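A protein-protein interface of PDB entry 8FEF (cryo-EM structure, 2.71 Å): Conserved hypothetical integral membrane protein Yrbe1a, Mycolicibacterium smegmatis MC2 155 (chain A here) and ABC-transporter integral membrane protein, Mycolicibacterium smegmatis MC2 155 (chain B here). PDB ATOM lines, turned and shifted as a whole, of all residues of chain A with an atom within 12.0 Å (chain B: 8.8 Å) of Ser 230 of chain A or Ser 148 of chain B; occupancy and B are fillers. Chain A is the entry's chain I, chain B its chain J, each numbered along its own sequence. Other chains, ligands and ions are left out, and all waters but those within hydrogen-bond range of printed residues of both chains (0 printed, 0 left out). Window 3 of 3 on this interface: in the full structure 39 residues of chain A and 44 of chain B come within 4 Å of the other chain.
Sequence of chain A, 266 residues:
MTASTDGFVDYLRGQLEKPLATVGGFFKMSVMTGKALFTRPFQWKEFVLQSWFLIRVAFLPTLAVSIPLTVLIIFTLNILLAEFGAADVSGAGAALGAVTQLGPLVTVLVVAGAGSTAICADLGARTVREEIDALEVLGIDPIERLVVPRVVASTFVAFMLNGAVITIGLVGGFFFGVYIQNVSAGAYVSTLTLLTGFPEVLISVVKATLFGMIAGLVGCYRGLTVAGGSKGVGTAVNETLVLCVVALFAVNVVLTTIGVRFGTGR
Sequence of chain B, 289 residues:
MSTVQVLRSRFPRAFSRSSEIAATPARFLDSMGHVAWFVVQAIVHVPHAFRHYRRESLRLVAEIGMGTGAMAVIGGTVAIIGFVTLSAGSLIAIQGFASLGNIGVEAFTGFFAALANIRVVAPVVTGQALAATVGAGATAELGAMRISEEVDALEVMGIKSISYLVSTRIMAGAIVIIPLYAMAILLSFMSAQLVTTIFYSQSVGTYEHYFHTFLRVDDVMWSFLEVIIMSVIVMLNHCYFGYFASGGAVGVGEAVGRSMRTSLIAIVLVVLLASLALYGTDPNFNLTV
Ala 125 of chain A touches Val 250 of chain B. Val 250 of chain B touches Arg 129 of chain A. Ile 147 of chain B touches Ser 230 of chain A. Ser 230 of chain A touches Ala 249 of chain B. Lys 231 of chain A touches Ala 140 of chain B. Lys 231 of chain A touches Ala 144 of chain B. O of Ala 249 of chain B touches CB of Val 233 of chain A (3.3 Å). Val 237 of chain A touches Gly 253 of chain B.
No residue of chain B comes within 4 Å of Gly 229 of chain A. Ile 147 of chain B touches just one residue of chain A: Ser 230 (3.9 Å). No residue of chain A comes within 4 Å of Glu 149 of chain B. No residue of chain A comes within 4 Å of Glu 150 of chain B. Gly 248 of chain B touches none of the printed residues of chain A. Printed residues of chain A within 4 Å of Val 250 of chain B: Ala 125 (3.7 Å) and Arg 129 (3.9 Å). Printed residues of chain B within 4 Å of Lys 231 of chain A: Ala 140, Glu 141 and Ala 144. Of the printed residues of chain A, Gly 253 of chain B touches Val 237 (3.7 Å). Printed residues of chain B within 4 Å of Val 237 of chain A: Gly 253 (3.7 Å). Ala 227 of chain A touches none of the printed residues of chain B. The nearest residue of chain B that does not touch Ser 230 of chain A is Ala 144 of chain B (4.2 Å). The nearest printed residue of chain A that does not touch Ala 140 of chain B is Gly 234 of chain A (4.3 Å).
Among the printed residues, 10 pairs touch across the chains. Among the printed residues, Asp or Glu carboxylates within 4 Å of a Lys or Arg side-chain nitrogen of the other chain: Lys 231 of chain A with Glu 141 of chain B.
The side-chain amino group (NZ) of Lys 231 of chain A lies within salt-bridge range of the side-chain carboxylate (OE2) of Glu 141 of chain B (2.6 Å). The side-chain hydroxyl (OG) of Ser 148 of chain B is in hydrogen-bond range of the side-chain hydroxyl (OG) of Ser 230 of chain A, at 3.3 Å.
The backbone carbonyl oxygen (O) of Lys 231 of chain A sits at hydrogen-bond distance from the side-chain hydroxyl (OG1) of Thr 235 of chain A (2.7 Å). The backbone carbonyl oxygen (O) of Ala 144 of chain B is in hydrogen-bond range of the side-chain hydroxyl (OG) of Ser 148 of chain B (2.9 Å).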
ATOM      1  N   GLY A 124      10.061 -23.502  21.903  1.00  0.00           N
ATOM      2  CA  GLY A 124       9.181 -23.586  20.751  1.00  0.00           C
ATOM      3  C   GLY A 124       8.534 -22.255  20.423  1.00  0.00           C
ATOM      4  O   GLY A 124       8.353 -21.916  19.252  1.00  0.00           O
ATOM      5  N   ALA A 125       8.169 -21.487  21.453  1.00  0.00           N
ATOM      6  CA  ALA A 125       7.648 -20.143  21.234  1.00  0.00           C
ATOM      7  C   ALA A 125       8.698 -19.248  20.594  1.00  0.00           C
ATOM      8  O   ALA A 125       8.385 -18.447  19.707  1.00  0.00           O
ATOM      9  CB  ALA A 125       7.169 -19.546  22.555  1.00  0.00           C
ATOM     10  N   THR A 127      11.110 -20.323  18.679  1.00  0.00           N
ATOM     11  CA  THR A 127      11.328 -20.815  17.323  1.00  0.00           C
ATOM     12  C   THR A 127      10.221 -20.361  16.376  1.00  0.00           C
ATOM     13  O   THR A 127      10.499 -19.874  15.274  1.00  0.00           O
ATOM     14  CB  THR A 127      11.435 -22.339  17.331  1.00  0.00           C
ATOM     15  OG1 THR A 127      12.561 -22.734  18.124  1.00  0.00           O
ATOM     16  CG2 THR A 127      11.616 -22.868  15.921  1.00  0.00           C
ATOM     17  N   VAL A 128       8.956 -20.512  16.785  1.00  0.00           N
ATOM     18  CA  VAL A 128       7.849 -20.162  15.899  1.00  0.00           C
ATOM     19  C   VAL A 128       7.756 -18.660  15.671  1.00  0.00           C
ATOM     20  O   VAL A 128       7.197 -18.228  14.657  1.00  0.00           O
ATOM     21  CB  VAL A 128       6.510 -20.706  16.433  1.00  0.00           C
ATOM     22  CG1 VAL A 128       6.561 -22.219  16.560  1.00  0.00           C
ATOM     23  CG2 VAL A 128       6.145 -20.057  17.758  1.00  0.00           C
ATOM     24  N   ARG A 129       8.289 -17.851  16.581  1.00  0.00           N
ATOM     25  CA  ARG A 129       8.327 -16.406  16.418  1.00  0.00           C
ATOM     26  C   ARG A 129       9.595 -15.936  15.722  1.00  0.00           C
ATOM     27  O   ARG A 129       9.843 -14.728  15.665  1.00  0.00           O
ATOM     28  CB  ARG A 129       8.185 -15.718  17.777  1.00  0.00           C
ATOM     29  CG  ARG A 129       6.834 -15.943  18.430  1.00  0.00           C
ATOM     30  CD  ARG A 129       6.844 -15.526  19.889  1.00  0.00           C
ATOM     31  NE  ARG A 129       5.555 -15.763  20.526  1.00  0.00           N
ATOM     32  CZ  ARG A 129       5.331 -15.656  21.828  1.00  0.00           C
ATOM     33  NH1 ARG A 129       6.297 -15.330  22.671  1.00  0.00           N
ATOM     34  NH2 ARG A 129       4.109 -15.884  22.297  1.00  0.00           N
ATOM     35  N   ARG A 222      13.839 -30.549  22.022  1.00  0.00           N
ATOM     36  CA  ARG A 222      12.507 -30.563  21.429  1.00  0.00           C
ATOM     37  C   ARG A 222      11.983 -29.156  21.177  1.00  0.00           C
ATOM     38  O   ARG A 222      11.267 -28.936  20.195  1.00  0.00           O
ATOM     39  CB  ARG A 222      11.540 -31.342  22.314  1.00  0.00           C
ATOM     40  CG  ARG A 222      11.627 -32.851  22.159  1.00  0.00           C
ATOM     41  CD  ARG A 222      11.453 -33.263  20.708  1.00  0.00           C
ATOM     42  NE  ARG A 222      10.236 -32.710  20.127  1.00  0.00           N
ATOM     43  CZ  ARG A 222       9.947 -32.735  18.832  1.00  0.00           C
ATOM     44  NH1 ARG A 222      10.768 -33.281  17.952  1.00  0.00           N
ATOM     45  NH2 ARG A 222       8.807 -32.194  18.412  1.00  0.00           N
ATOM     46  N   VAL A 226      10.832 -27.477  17.007  1.00  0.00           N
ATOM     47  CA  VAL A 226       9.376 -27.505  16.957  1.00  0.00           C
ATOM     48  C   VAL A 226       8.910 -27.358  15.510  1.00  0.00           C
ATOM     49  O   VAL A 226       9.605 -26.787  14.658  1.00  0.00           O
ATOM     50  CB  VAL A 226       8.784 -26.409  17.864  1.00  0.00           C
ATOM     51  CG1 VAL A 226       8.885 -25.046  17.211  1.00  0.00           C
ATOM     52  CG2 VAL A 226       7.352 -26.730  18.236  1.00  0.00           C
ATOM     53  N   ALA A 227       7.729 -27.904  15.220  1.00  0.00           N
ATOM     54  CA  ALA A 227       7.199 -27.962  13.863  1.00  0.00           C
ATOM     55  C   ALA A 227       6.263 -26.810  13.520  1.00  0.00           C
ATOM     56  O   ALA A 227       5.779 -26.747  12.385  1.00  0.00           O
ATOM     57  CB  ALA A 227       6.469 -29.290  13.642  1.00  0.00           C
ATOM     58  N   GLY A 228       6.002 -25.898  14.453  1.00  0.00           N
ATOM     59  CA  GLY A 228       5.126 -24.774  14.180  1.00  0.00           C
ATOM     60  C   GLY A 228       3.689 -25.190  13.947  1.00  0.00           C
ATOM     61  O   GLY A 228       3.084 -25.832  14.809  1.00  0.00           O
ATOM     62  N   GLY A 229       3.131 -24.829  12.792  1.00  0.00           N
ATOM     63  CA  GLY A 229       1.755 -25.188  12.484  1.00  0.00           C
ATOM     64  C   GLY A 229       0.772 -24.618  13.487  1.00  0.00           C
ATOM     65  O   GLY A 229       0.879 -23.466  13.920  1.00  0.00           O
ATOM     66  N   SER A 230      -0.210 -25.440  13.862  1.00  0.00           N
ATOM     67  CA  SER A 230      -1.164 -25.093  14.904  1.00  0.00           C
ATOM     68  C   SER A 230      -1.179 -26.080  16.061  1.00  0.00           C
ATOM     69  O   SER A 230      -1.751 -25.767  17.110  1.00  0.00           O
ATOM     70  CB  SER A 230      -2.583 -24.983  14.325  1.00  0.00           C
ATOM     71  OG  SER A 230      -3.524 -24.696  15.344  1.00  0.00           O
ATOM     72  N   LYS A 231      -0.577 -27.258  15.899  1.00  0.00           N
ATOM     73  CA  LYS A 231      -0.441 -28.231  16.976  1.00  0.00           C
ATOM     74  C   LYS A 231       1.015 -28.630  17.190  1.00  0.00           C
ATOM     75  O   LYS A 231       1.291 -29.552  17.965  1.00  0.00           O
ATOM     76  CB  LYS A 231      -1.299 -29.466  16.672  1.00  0.00           C
ATOM     77  CG  LYS A 231      -1.655 -30.329  17.876  1.00  0.00           C
ATOM     78  CD  LYS A 231      -2.256 -31.650  17.437  1.00  0.00           C
ATOM     79  CE  LYS A 231      -2.425 -32.593  18.611  1.00  0.00           C
ATOM     80  NZ  LYS A 231      -2.899 -33.931  18.168  1.00  0.00           N
ATOM     81  N   GLY A 232       1.956 -27.953  16.531  1.00  0.00           N
ATOM     82  CA  GLY A 232       3.350 -28.352  16.629  1.00  0.00           C
ATOM     83  C   GLY A 232       3.933 -28.162  18.015  1.00  0.00           C
ATOM     84  O   GLY A 232       4.691 -29.006  18.497  1.00  0.00           O
ATOM     85  N   VAL A 233       3.599 -27.050  18.672  1.00  0.00           N
ATOM     86  CA  VAL A 233       4.152 -26.785  19.997  1.00  0.00           C
ATOM     87  C   VAL A 233       3.570 -27.747  21.025  1.00  0.00           C
ATOM     88  O   VAL A 233       4.297 -28.281  21.871  1.00  0.00           O
ATOM     89  CB  VAL A 233       3.921 -25.316  20.392  1.00  0.00           C
ATOM     90  CG1 VAL A 233       4.551 -25.025  21.743  1.00  0.00           C
ATOM     91  CG2 VAL A 233       4.488 -24.390  19.333  1.00  0.00           C
ATOM     92  N   GLY A 234       2.259 -27.988  20.971  1.00  0.00           N
ATOM     93  CA  GLY A 234       1.655 -28.943  21.888  1.00  0.00           C
ATOM     94  C   GLY A 234       2.158 -30.358  21.673  1.00  0.00           C
ATOM     95  O   GLY A 234       2.413 -31.091  22.633  1.00  0.00           O
ATOM     96  N   THR A 235       2.307 -30.759  20.407  1.00  0.00           N
ATOM     97  CA  THR A 235       2.873 -32.069  20.104  1.00  0.00           C
ATOM     98  C   THR A 235       4.305 -32.175  20.609  1.00  0.00           C
ATOM     99  O   THR A 235       4.704 -33.210  21.156  1.00  0.00           O
ATOM    100  CB  THR A 235       2.817 -32.329  18.599  1.00  0.00           C
ATOM    101  OG1 THR A 235       1.460 -32.237  18.149  1.00  0.00           O
ATOM    102  CG2 THR A 235       3.358 -33.710  18.270  1.00  0.00           C
ATOM    103  N   ALA A 236       5.093 -31.110  20.436  1.00  0.00           N
ATOM    104  CA  ALA A 236       6.467 -31.112  20.921  1.00  0.00           C
ATOM    105  C   ALA A 236       6.520 -31.235  22.437  1.00  0.00           C
ATOM    106  O   ALA A 236       7.355 -31.967  22.974  1.00  0.00           O
ATOM    107  CB  ALA A 236       7.186 -29.845  20.458  1.00  0.00           C
ATOM    108  N   VAL A 237       5.636 -30.528  23.142  1.00  0.00           N
ATOM    109  CA  VAL A 237       5.608 -30.610  24.601  1.00  0.00           C
ATOM    110  C   VAL A 237       5.213 -32.012  25.057  1.00  0.00           C
ATOM    111  O   VAL A 237       5.809 -32.569  25.990  1.00  0.00           O
ATOM    112  CB  VAL A 237       4.669 -29.535  25.177  1.00  0.00           C
ATOM    113  CG1 VAL A 237       4.475 -29.738  26.661  1.00  0.00           C
ATOM    114  CG2 VAL A 237       5.235 -28.154  24.918  1.00  0.00           C
ATOM    115  N   ASN A 238       4.204 -32.603  24.410  1.00  0.00           N
ATOM    116  CA  ASN A 238       3.779 -33.953  24.771  1.00  0.00           C
ATOM    117  C   ASN A 238       4.891 -34.970  24.525  1.00  0.00           C
ATOM    118  O   ASN A 238       5.141 -35.846  25.365  1.00  0.00           O
ATOM    119  CB  ASN A 238       2.519 -34.319  23.987  1.00  0.00           C
ATOM    120  CG  ASN A 238       1.941 -35.661  24.392  1.00  0.00           C
ATOM    121  OD1 ASN A 238       2.284 -36.213  25.436  1.00  0.00           O
ATOM    122  ND2 ASN A 238       1.047 -36.187  23.567  1.00  0.00           N
ATOM    123  N   ALA B 140      -3.605 -31.455  23.997  1.00  0.00           N
ATOM    124  CA  ALA B 140      -3.083 -30.927  22.742  1.00  0.00           C
ATOM    125  C   ALA B 140      -4.147 -30.936  21.651  1.00  0.00           C
ATOM    126  O   ALA B 140      -4.286 -29.959  20.907  1.00  0.00           O
ATOM    127  CB  ALA B 140      -1.858 -31.728  22.305  1.00  0.00           C
ATOM    128  N   GLU B 141      -4.911 -32.028  21.543  1.00  0.00           N
ATOM    129  CA  GLU B 141      -5.948 -32.117  20.518  1.00  0.00           C
ATOM    130  C   GLU B 141      -7.028 -31.064  20.728  1.00  0.00           C
ATOM    131  O   GLU B 141      -7.428 -30.374  19.783  1.00  0.00           O
ATOM    132  CB  GLU B 141      -6.565 -33.515  20.515  1.00  0.00           C
ATOM    133  CG  GLU B 141      -5.873 -34.504  19.599  1.00  0.00           C
ATOM    134  CD  GLU B 141      -6.072 -34.177  18.132  1.00  0.00           C
ATOM    135  OE1 GLU B 141      -7.079 -33.519  17.797  1.00  0.00           O
ATOM    136  OE2 GLU B 141      -5.218 -34.577  17.313  1.00  0.00           O
ATOM    137  N   LEU B 142      -7.511 -30.922  21.963  1.00  0.00           N
ATOM    138  CA  LEU B 142      -8.572 -29.957  22.225  1.00  0.00           C
ATOM    139  C   LEU B 142      -8.070 -28.526  22.080  1.00  0.00           C
ATOM    140  O   LEU B 142      -8.809 -27.653  21.613  1.00  0.00           O
ATOM    141  CB  LEU B 142      -9.176 -30.194  23.607  1.00  0.00           C
ATOM    142  CG  LEU B 142      -9.904 -31.527  23.796  1.00  0.00           C
ATOM    143  CD1 LEU B 142     -10.683 -31.530  25.093  1.00  0.00           C
ATOM    144  CD2 LEU B 142     -10.822 -31.821  22.624  1.00  0.00           C
ATOM    145  N   GLY B 143      -6.817 -28.262  22.458  1.00  0.00           N
ATOM    146  CA  GLY B 143      -6.254 -26.944  22.228  1.00  0.00           C
ATOM    147  C   GLY B 143      -6.106 -26.621  20.754  1.00  0.00           C
ATOM    148  O   GLY B 143      -6.384 -25.499  20.326  1.00  0.00           O
ATOM    149  N   ALA B 144      -5.667 -27.598  19.956  1.00  0.00           N
ATOM    150  CA  ALA B 144      -5.568 -27.390  18.517  1.00  0.00           C
ATOM    151  C   ALA B 144      -6.938 -27.142  17.902  1.00  0.00           C
ATOM    152  O   ALA B 144      -7.079 -26.304  17.004  1.00  0.00           O
ATOM    153  CB  ALA B 144      -4.895 -28.592  17.858  1.00  0.00           C
ATOM    154  N   MET B 145      -7.958 -27.871  18.362  1.00  0.00           N
ATOM    155  CA  MET B 145      -9.315 -27.635  17.876  1.00  0.00           C
ATOM    156  C   MET B 145      -9.807 -26.247  18.264  1.00  0.00           C
ATOM    157  O   MET B 145     -10.454 -25.565  17.462  1.00  0.00           O
ATOM    158  CB  MET B 145     -10.261 -28.708  18.411  1.00  0.00           C
ATOM    159  CG  MET B 145      -9.997 -30.094  17.857  1.00  0.00           C
ATOM    160  SD  MET B 145     -11.111 -31.339  18.523  1.00  0.00           S
ATOM    161  CE  MET B 145     -10.479 -32.812  17.727  1.00  0.00           C
ATOM    162  N   ARG B 146      -9.523 -25.818  19.495  1.00  0.00           N
ATOM    163  CA  ARG B 146      -9.939 -24.491  19.938  1.00  0.00           C
ATOM    164  C   ARG B 146      -9.262 -23.397  19.122  1.00  0.00           C
ATOM    165  O   ARG B 146      -9.907 -22.420  18.724  1.00  0.00           O
ATOM    166  CB  ARG B 146      -9.633 -24.323  21.424  1.00  0.00           C
ATOM    167  CG  ARG B 146      -9.825 -22.914  21.948  1.00  0.00           C
ATOM    168  CD  ARG B 146     -11.278 -22.492  21.869  1.00  0.00           C
ATOM    169  NE  ARG B 146     -12.128 -23.280  22.752  1.00  0.00           N
ATOM    170  CZ  ARG B 146     -13.431 -23.089  22.899  1.00  0.00           C
ATOM    171  NH1 ARG B 146     -14.071 -22.147  22.226  1.00  0.00           N
ATOM    172  NH2 ARG B 146     -14.109 -23.861  23.742  1.00  0.00           N
ATOM    173  N   ILE B 147      -7.961 -23.540  18.863  1.00  0.00           N
ATOM    174  CA  ILE B 147      -7.230 -22.516  18.123  1.00  0.00           C
ATOM    175  C   ILE B 147      -7.659 -22.495  16.661  1.00  0.00           C
ATOM    176  O   ILE B 147      -7.845 -21.425  16.070  1.00  0.00           O
ATOM    177  CB  ILE B 147      -5.713 -22.732  18.275  1.00  0.00           C
ATOM    178  CG1 ILE B 147      -5.304 -22.578  19.741  1.00  0.00           C
ATOM    179  CG2 ILE B 147      -4.938 -21.762  17.404  1.00  0.00           C
ATOM    180  CD1 ILE B 147      -5.787 -21.296  20.379  1.00  0.00           C
ATOM    181  N   SER B 148      -7.842 -23.670  16.058  1.00  0.00           N
ATOM    182  CA  SER B 148      -8.236 -23.777  14.658  1.00  0.00           C
ATOM    183  C   SER B 148      -9.711 -23.471  14.424  1.00  0.00           C
ATOM    184  O   SER B 148     -10.201 -23.712  13.316  1.00  0.00           O
ATOM    185  CB  SER B 148      -7.913 -25.173  14.123  1.00  0.00           C
ATOM    186  OG  SER B 148      -6.533 -25.461  14.254  1.00  0.00           O
ATOM    187  N   GLU B 149     -10.419 -22.968  15.440  1.00  0.00           N
ATOM    188  CA  GLU B 149     -11.829 -22.583  15.343  1.00  0.00           C
ATOM    189  C   GLU B 149     -12.730 -23.763  14.988  1.00  0.00           C
ATOM    190  O   GLU B 149     -13.808 -23.582  14.417  1.00  0.00           O
ATOM    191  CB  GLU B 149     -12.027 -21.439  14.343  1.00  0.00           C
ATOM    192  CG  GLU B 149     -11.311 -20.157  14.730  1.00  0.00           C
ATOM    193  CD  GLU B 149     -11.183 -19.189  13.572  1.00  0.00           C
ATOM    194  OE1 GLU B 149     -11.252 -19.637  12.409  1.00  0.00           O
ATOM    195  OE2 GLU B 149     -11.011 -17.977  13.824  1.00  0.00           O
ATOM    196  N   GLU B 150     -12.301 -24.983  15.314  1.00  0.00           N
ATOM    197  CA  GLU B 150     -13.141 -26.149  15.062  1.00  0.00           C
ATOM    198  C   GLU B 150     -14.263 -26.270  16.084  1.00  0.00           C
ATOM    199  O   GLU B 150     -15.340 -26.778  15.756  1.00  0.00           O
ATOM    200  CB  GLU B 150     -12.291 -27.417  15.048  1.00  0.00           C
ATOM    201  CG  GLU B 150     -11.217 -27.419  13.975  1.00  0.00           C
ATOM    202  CD  GLU B 150     -10.423 -28.707  13.943  1.00  0.00           C
ATOM    203  OE1 GLU B 150     -10.851 -29.688  14.588  1.00  0.00           O
ATOM    204  OE2 GLU B 150      -9.370 -28.741  13.276  1.00  0.00           O
ATOM    205  N   VAL B 151     -14.034 -25.814  17.316  1.00  0.00           N
ATOM    206  CA  VAL B 151     -15.108 -25.770  18.303  1.00  0.00           C
ATOM    207  C   VAL B 151     -16.168 -24.761  17.881  1.00  0.00           C
ATOM    208  O   VAL B 151     -17.373 -24.999  18.041  1.00  0.00           O
ATOM    209  CB  VAL B 151     -14.535 -25.456  19.698  1.00  0.00           C
ATOM    210  CG1 VAL B 151     -15.651 -25.330  20.720  1.00  0.00           C
ATOM    211  CG2 VAL B 151     -13.550 -26.532  20.115  1.00  0.00           C
ATOM    212  N   ASP B 152     -15.740 -23.623  17.328  1.00  0.00           N
ATOM    213  CA  ASP B 152     -16.686 -22.667  16.764  1.00  0.00           C
ATOM    214  C   ASP B 152     -17.450 -23.276  15.597  1.00  0.00           C
ATOM    215  O   ASP B 152     -18.649 -23.027  15.435  1.00  0.00           O
ATOM    216  CB  ASP B 152     -15.959 -21.398  16.321  1.00  0.00           C
ATOM    217  CG  ASP B 152     -15.561 -20.519  17.485  1.00  0.00           C
ATOM    218  OD1 ASP B 152     -15.876 -20.879  18.637  1.00  0.00           O
ATOM    219  OD2 ASP B 152     -14.935 -19.465  17.247  1.00  0.00           O
ATOM    220  N   ALA B 153     -16.768 -24.066  14.765  1.00  0.00           N
ATOM    221  CA  ALA B 153     -17.443 -24.731  13.655  1.00  0.00           C
ATOM    222  C   ALA B 153     -18.500 -25.704  14.158  1.00  0.00           C
ATOM    223  O   ALA B 153     -19.592 -25.796  13.587  1.00  0.00           O
ATOM    224  CB  ALA B 153     -16.424 -25.453  12.774  1.00  0.00           C
ATOM    225  N   LEU B 154     -18.187 -26.451  15.220  1.00  0.00           N
ATOM    226  CA  LEU B 154     -19.165 -27.363  15.805  1.00  0.00           C
ATOM    227  C   LEU B 154     -20.349 -26.605  16.394  1.00  0.00           C
ATOM    228  O   LEU B 154     -21.502 -27.017  16.227  1.00  0.00           O
ATOM    229  CB  LEU B 154     -18.502 -28.231  16.871  1.00  0.00           C
ATOM    230  CG  LEU B 154     -17.612 -29.366  16.369  1.00  0.00           C
ATOM    231  CD1 LEU B 154     -16.895 -30.032  17.528  1.00  0.00           C
ATOM    232  CD2 LEU B 154     -18.440 -30.379  15.602  1.00  0.00           C
ATOM    233  N   ALA B 245      -8.316 -23.545  25.942  1.00  0.00           N
ATOM    234  CA  ALA B 245      -6.992 -23.035  25.629  1.00  0.00           C
ATOM    235  C   ALA B 245      -7.088 -21.691  24.913  1.00  0.00           C
ATOM    236  O   ALA B 245      -8.103 -21.351  24.300  1.00  0.00           O
ATOM    237  CB  ALA B 245      -6.222 -24.034  24.766  1.00  0.00           C
ATOM    238  N   GLY B 247      -4.282 -18.288  23.226  1.00  0.00           N
ATOM    239  CA  GLY B 247      -2.947 -17.824  22.919  1.00  0.00           C
ATOM    240  C   GLY B 247      -2.294 -18.464  21.718  1.00  0.00           C
ATOM    241  O   GLY B 247      -1.064 -18.422  21.610  1.00  0.00           O
ATOM    242  N   GLY B 248      -3.070 -19.052  20.812  1.00  0.00           N
ATOM    243  CA  GLY B 248      -2.485 -19.654  19.633  1.00  0.00           C
ATOM    244  C   GLY B 248      -1.765 -20.952  19.959  1.00  0.00           C
ATOM    245  O   GLY B 248      -2.016 -21.605  20.973  1.00  0.00           O
ATOM    246  N   ALA B 249      -0.848 -21.325  19.062  1.00  0.00           N
ATOM    247  CA  ALA B 249      -0.093 -22.561  19.229  1.00  0.00           C
ATOM    248  C   ALA B 249       0.818 -22.529  20.450  1.00  0.00           C
ATOM    249  O   ALA B 249       1.162 -23.592  20.976  1.00  0.00           O
ATOM    250  CB  ALA B 249       0.731 -22.847  17.974  1.00  0.00           C
ATOM    251  N   VAL B 250       1.215 -21.340  20.904  1.00  0.00           N
ATOM    252  CA  VAL B 250       2.117 -21.234  22.046  1.00  0.00           C
ATOM    253  C   VAL B 250       1.407 -21.635  23.336  1.00  0.00           C
ATOM    254  O   VAL B 250       1.988 -22.311  24.194  1.00  0.00           O
ATOM    255  CB  VAL B 250       2.692 -19.809  22.131  1.00  0.00           C
ATOM    256  CG1 VAL B 250       3.596 -19.665  23.343  1.00  0.00           C
ATOM    257  CG2 VAL B 250       3.444 -19.470  20.856  1.00  0.00           C
ATOM    258  N   GLY B 251       0.143 -21.236  23.491  1.00  0.00           N
ATOM    259  CA  GLY B 251      -0.583 -21.505  24.722  1.00  0.00           C
ATOM    260  C   GLY B 251      -0.909 -22.966  24.950  1.00  0.00           C
ATOM    261  O   GLY B 251      -1.155 -23.364  26.096  1.00  0.00           O
ATOM    262  N   VAL B 252      -0.917 -23.772  23.886  1.00  0.00           N
ATOM    263  CA  VAL B 252      -1.247 -25.188  24.018  1.00  0.00           C
ATOM    264  C   VAL B 252      -0.207 -25.907  24.872  1.00  0.00           C
ATOM    265  O   VAL B 252      -0.550 -26.740  25.719  1.00  0.00           O
ATOM    266  CB  VAL B 252      -1.390 -25.831  22.627  1.00  0.00           C
ATOM    267  CG1 VAL B 252      -1.875 -27.264  22.752  1.00  0.00           C
ATOM    268  CG2 VAL B 252      -2.344 -25.020  21.769  1.00  0.00           C
ATOM    269  N   GLY B 253       1.077 -25.594  24.671  1.00  0.00           N
ATOM    270  CA  GLY B 253       2.117 -26.226  25.472  1.00  0.00           C
ATOM    271  C   GLY B 253       2.033 -25.861  26.943  1.00  0.00           C
ATOM    272  O   GLY B 253       2.233 -26.709  27.821  1.00  0.00           O
